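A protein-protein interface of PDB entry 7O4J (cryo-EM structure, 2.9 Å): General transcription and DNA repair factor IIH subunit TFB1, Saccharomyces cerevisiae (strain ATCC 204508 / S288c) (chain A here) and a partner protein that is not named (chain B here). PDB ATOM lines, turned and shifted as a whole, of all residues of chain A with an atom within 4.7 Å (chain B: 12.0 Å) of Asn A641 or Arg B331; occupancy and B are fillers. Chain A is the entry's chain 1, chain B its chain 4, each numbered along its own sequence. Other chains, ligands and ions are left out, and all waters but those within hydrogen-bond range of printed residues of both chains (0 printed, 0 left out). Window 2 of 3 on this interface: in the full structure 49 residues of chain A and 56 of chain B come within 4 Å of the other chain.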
ATOM      1  N   GLN A 576      -4.741   7.854  -5.809  1.00  0.00           N
ATOM      2  CA  GLN A 576      -4.854   6.584  -6.515  1.00  0.00           C
ATOM      3  C   GLN A 576      -5.768   5.588  -5.812  1.00  0.00           C
ATOM      4  O   GLN A 576      -5.982   4.492  -6.340  1.00  0.00           O
ATOM      5  CB  GLN A 576      -3.466   5.969  -6.706  1.00  0.00           C
ATOM      6  CG  GLN A 576      -2.754   6.449  -7.963  1.00  0.00           C
ATOM      7  CD  GLN A 576      -2.958   5.524  -9.147  1.00  0.00           C
ATOM      8  OE1 GLN A 576      -3.643   4.506  -9.046  1.00  0.00           O
ATOM      9  NE2 GLN A 576      -2.365   5.876 -10.282  1.00  0.00           N
ATOM     10  N   PHE A 637      -2.955   5.633 -19.459  1.00  0.00           N
ATOM     11  CA  PHE A 637      -2.765   4.248 -19.044  1.00  0.00           C
ATOM     12  C   PHE A 637      -1.547   3.637 -19.723  1.00  0.00           C
ATOM     13  O   PHE A 637      -0.780   2.895 -19.099  1.00  0.00           O
ATOM     14  CB  PHE A 637      -4.022   3.434 -19.353  1.00  0.00           C
ATOM     15  CG  PHE A 637      -3.899   1.976 -19.015  1.00  0.00           C
ATOM     16  CD1 PHE A 637      -4.028   1.540 -17.707  1.00  0.00           C
ATOM     17  CD2 PHE A 637      -3.654   1.040 -20.007  1.00  0.00           C
ATOM     18  CE1 PHE A 637      -3.915   0.199 -17.394  1.00  0.00           C
ATOM     19  CE2 PHE A 637      -3.541  -0.302 -19.699  1.00  0.00           C
ATOM     20  CZ  PHE A 637      -3.671  -0.724 -18.392  1.00  0.00           C
ATOM     21  N   ASN A 638      -1.353   3.938 -21.008  1.00  0.00           N
ATOM     22  CA  ASN A 638      -0.228   3.376 -21.747  1.00  0.00           C
ATOM     23  C   ASN A 638       1.100   3.793 -21.124  1.00  0.00           C
ATOM     24  O   ASN A 638       1.955   2.953 -20.826  1.00  0.00           O
ATOM     25  CB  ASN A 638      -0.302   3.813 -23.211  1.00  0.00           C
ATOM     26  CG  ASN A 638      -1.339   3.037 -23.998  1.00  0.00           C
ATOM     27  OD1 ASN A 638      -2.127   2.280 -23.431  1.00  0.00           O
ATOM     28  ND2 ASN A 638      -1.346   3.226 -25.313  1.00  0.00           N
ATOM     29  N   GLU A 639       1.288   5.099 -20.917  1.00  0.00           N
ATOM     30  CA  GLU A 639       2.542   5.577 -20.343  1.00  0.00           C
ATOM     31  C   GLU A 639       2.738   5.050 -18.928  1.00  0.00           C
ATOM     32  O   GLU A 639       3.846   4.645 -18.555  1.00  0.00           O
ATOM     33  CB  GLU A 639       2.577   7.107 -20.348  1.00  0.00           C
ATOM     34  CG  GLU A 639       2.100   7.747 -21.644  1.00  0.00           C
ATOM     35  CD  GLU A 639       2.616   7.032 -22.877  1.00  0.00           C
ATOM     36  OE1 GLU A 639       3.851   6.984 -23.066  1.00  0.00           O
ATOM     37  OE2 GLU A 639       1.788   6.516 -23.656  1.00  0.00           O
ATOM     38  N   TYR A 640       1.676   5.047 -18.124  1.00  0.00           N
ATOM     39  CA  TYR A 640       1.775   4.655 -16.725  1.00  0.00           C
ATOM     40  C   TYR A 640       2.037   3.163 -16.567  1.00  0.00           C
ATOM     41  O   TYR A 640       3.072   2.763 -16.022  1.00  0.00           O
ATOM     42  CB  TYR A 640       0.494   5.042 -15.982  1.00  0.00           C
ATOM     43  CG  TYR A 640       0.423   4.512 -14.571  1.00  0.00           C
ATOM     44  CD1 TYR A 640       1.141   5.111 -13.544  1.00  0.00           C
ATOM     45  CD2 TYR A 640      -0.362   3.410 -14.263  1.00  0.00           C
ATOM     46  CE1 TYR A 640       1.077   4.627 -12.251  1.00  0.00           C
ATOM     47  CE2 TYR A 640      -0.431   2.919 -12.977  1.00  0.00           C
ATOM     48  CZ  TYR A 640       0.290   3.531 -11.974  1.00  0.00           C
ATOM     49  OH  TYR A 640       0.220   3.042 -10.690  1.00  0.00           O
ATOM     50  N   ASN A 641       1.108   2.328 -17.041  1.00  0.00           N
ATOM     51  CA  ASN A 641       1.214   0.894 -16.794  1.00  0.00           C
ATOM     52  C   ASN A 641       2.355   0.271 -17.590  1.00  0.00           C
ATOM     53  O   ASN A 641       3.140  -0.517 -17.049  1.00  0.00           O
ATOM     54  CB  ASN A 641      -0.109   0.206 -17.132  1.00  0.00           C
ATOM     55  CG  ASN A 641      -0.173  -1.219 -16.615  1.00  0.00           C
ATOM     56  OD1 ASN A 641       0.399  -1.540 -15.574  1.00  0.00           O
ATOM     57  ND2 ASN A 641      -0.873  -2.082 -17.343  1.00  0.00           N
ATOM     58  N   ASN A 642       2.464   0.607 -18.871  1.00  0.00           N
ATOM     59  CA  ASN A 642       3.474  -0.001 -19.731  1.00  0.00           C
ATOM     60  C   ASN A 642       3.909   0.950 -20.840  1.00  0.00           C
ATOM     61  O   ASN A 642       4.873   1.698 -20.688  1.00  0.00           O
ATOM     62  CB  ASN A 642       2.939  -1.300 -20.337  1.00  0.00           C
ATOM     63  CG  ASN A 642       2.931  -2.446 -19.344  1.00  0.00           C
ATOM     64  OD1 ASN A 642       3.971  -3.027 -19.041  1.00  0.00           O
ATOM     65  ND2 ASN A 642       1.750  -2.773 -18.829  1.00  0.00           N
ATOM     66  N   ARG B 325      -0.321  17.241  -9.558  1.00  0.00           N
ATOM     67  CA  ARG B 325      -0.627  15.818  -9.528  1.00  0.00           C
ATOM     68  C   ARG B 325      -1.049  15.321 -10.905  1.00  0.00           C
ATOM     69  O   ARG B 325      -1.785  15.990 -11.637  1.00  0.00           O
ATOM     70  CB  ARG B 325      -1.732  15.526  -8.511  1.00  0.00           C
ATOM     71  CG  ARG B 325      -1.299  15.685  -7.062  1.00  0.00           C
ATOM     72  CD  ARG B 325      -1.851  14.565  -6.194  1.00  0.00           C
ATOM     73  NE  ARG B 325      -1.921  14.939  -4.783  1.00  0.00           N
ATOM     74  CZ  ARG B 325      -3.035  15.284  -4.140  1.00  0.00           C
ATOM     75  NH1 ARG B 325      -4.205  15.306  -4.767  1.00  0.00           N
ATOM     76  NH2 ARG B 325      -2.979  15.606  -2.855  1.00  0.00           N
ATOM     77  N   LYS B 326      -0.569  14.130 -11.253  1.00  0.00           N
ATOM     78  CA  LYS B 326      -0.927  13.483 -12.502  1.00  0.00           C
ATOM     79  C   LYS B 326      -2.304  12.835 -12.395  1.00  0.00           C
ATOM     80  O   LYS B 326      -2.822  12.630 -11.296  1.00  0.00           O
ATOM     81  CB  LYS B 326       0.114  12.427 -12.869  1.00  0.00           C
ATOM     82  CG  LYS B 326       1.568  12.891 -12.769  1.00  0.00           C
ATOM     83  CD  LYS B 326       2.161  13.218 -14.135  1.00  0.00           C
ATOM     84  CE  LYS B 326       3.661  12.970 -14.165  1.00  0.00           C
ATOM     85  NZ  LYS B 326       4.206  12.973 -15.551  1.00  0.00           N
ATOM     86  N   PRO B 327      -2.922  12.505 -13.527  1.00  0.00           N
ATOM     87  CA  PRO B 327      -4.236  11.855 -13.484  1.00  0.00           C
ATOM     88  C   PRO B 327      -4.169  10.481 -12.836  1.00  0.00           C
ATOM     89  O   PRO B 327      -3.133   9.813 -12.820  1.00  0.00           O
ATOM     90  CB  PRO B 327      -4.637  11.750 -14.962  1.00  0.00           C
ATOM     91  CG  PRO B 327      -3.782  12.741 -15.671  1.00  0.00           C
ATOM     92  CD  PRO B 327      -2.499  12.792 -14.907  1.00  0.00           C
ATOM     93  N   VAL B 328      -5.309  10.064 -12.295  1.00  0.00           N
ATOM     94  CA  VAL B 328      -5.424   8.792 -11.588  1.00  0.00           C
ATOM     95  C   VAL B 328      -5.675   7.688 -12.606  1.00  0.00           C
ATOM     96  O   VAL B 328      -6.608   7.774 -13.412  1.00  0.00           O
ATOM     97  CB  VAL B 328      -6.545   8.841 -10.540  1.00  0.00           C
ATOM     98  CG1 VAL B 328      -6.943   7.434 -10.113  1.00  0.00           C
ATOM     99  CG2 VAL B 328      -6.113   9.665  -9.339  1.00  0.00           C
ATOM    100  N   VAL B 329      -4.843   6.652 -12.570  1.00  0.00           N
ATOM    101  CA  VAL B 329      -4.993   5.491 -13.444  1.00  0.00           C
ATOM    102  C   VAL B 329      -4.833   4.237 -12.593  1.00  0.00           C
ATOM    103  O   VAL B 329      -4.074   4.255 -11.613  1.00  0.00           O
ATOM    104  CB  VAL B 329      -3.972   5.530 -14.593  1.00  0.00           C
ATOM    105  CG1 VAL B 329      -4.074   4.283 -15.458  1.00  0.00           C
ATOM    106  CG2 VAL B 329      -4.172   6.780 -15.438  1.00  0.00           C
ATOM    107  N   PRO B 330      -5.512   3.133 -12.912  1.00  0.00           N
ATOM    108  CA  PRO B 330      -5.337   1.914 -12.113  1.00  0.00           C
ATOM    109  C   PRO B 330      -3.893   1.436 -12.116  1.00  0.00           C
ATOM    110  O   PRO B 330      -3.185   1.532 -13.121  1.00  0.00           O
ATOM    111  CB  PRO B 330      -6.268   0.906 -12.795  1.00  0.00           C
ATOM    112  CG  PRO B 330      -7.301   1.737 -13.460  1.00  0.00           C
ATOM    113  CD  PRO B 330      -6.601   2.990 -13.895  1.00  0.00           C
ATOM    114  N   ARG B 331      -3.464   0.914 -10.971  1.00  0.00           N
ATOM    115  CA  ARG B 331      -2.108   0.401 -10.813  1.00  0.00           C
ATOM    116  C   ARG B 331      -1.953  -0.943 -11.516  1.00  0.00           C
ATOM    117  O   ARG B 331      -0.871  -1.283 -11.993  1.00  0.00           O
ATOM    118  CB  ARG B 331      -1.757   0.264  -9.330  1.00  0.00           C
ATOM    119  CG  ARG B 331      -1.891   1.557  -8.539  1.00  0.00           C
ATOM    120  CD  ARG B 331      -1.769   1.312  -7.044  1.00  0.00           C
ATOM    121  NE  ARG B 331      -1.903   2.545  -6.274  1.00  0.00           N
ATOM    122  CZ  ARG B 331      -1.922   2.604  -4.946  1.00  0.00           C
ATOM    123  NH1 ARG B 331      -1.814   1.495  -4.225  1.00  0.00           N
ATOM    124  NH2 ARG B 331      -2.048   3.773  -4.334  1.00  0.00           N
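The side-chain amide nitrogen of Asn A642 sits close to the side-chain amide nitrogen of Asn A641 (3.1 Å).
Of the 7 printed residues of chain B, 3 touch a printed residue of chain A. Hydrophobic or aromatic side chains of chain B that line the printed part of chain A: Val B329. Of the 7 printed residues of chain A, 4 touch a printed residue of chain B. Along chain A the printed residues that touch a printed residue of chain B span positions 576 to 641. Among the printed residues, no Asp or Glu carboxylate lies within 4 Å of a Lys or Arg side-chain nitrogen of the other chain.
Of the printed residues of chain B, Gln A576 touches Val B329 and Arg B331. Of chain B, only Val B329 (3.5 Å) comes within 4 Å of Phe A637. Asn A638 touches none of the printed residues of chain B. Glu A639 touches none of the printed residues of chain B. Of the printed residues of chain B, Tyr A640 touches Val B329 (3.996 Å), Pro B330 (3.1 Å) and Arg B331 (3.4 Å). Of chain B, only Arg B331 (3.8 Å) comes within 4 Å of Asn A641. No residue of chain B comes within 4 Å of Asn A642. Printed residues of chain A within 4 Å of Val B329: Gln A576, Phe A637 and Tyr A640. Of the printed residues of chain A, Pro B330 touches Tyr A640. The nearest residue of chain B that does not touch Asn A641 is Pro B330 (5.2 Å).
Arg B331 touches Gln A576 (CG to OE1, 3.5 Å). CG1 of Val B329 touches CD1 of Phe A637, at 3.5 Å. Tyr A640 touches Val B329 (CD2 to CG1, 3.996 Å). Tyr A640 touches Pro B330 (CE2 to O, 3.1 Å). Arg B331 touches Tyr A640 (CG to OH, 3.4 Å). O of Arg B331 touches OD1 of Asn A641, 3.8 Å away.
The side-chain amide oxygen (OE1) of Gln A576 lies close to the backbone carbonyl oxygen (O) of Val B329 (2.6 Å).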
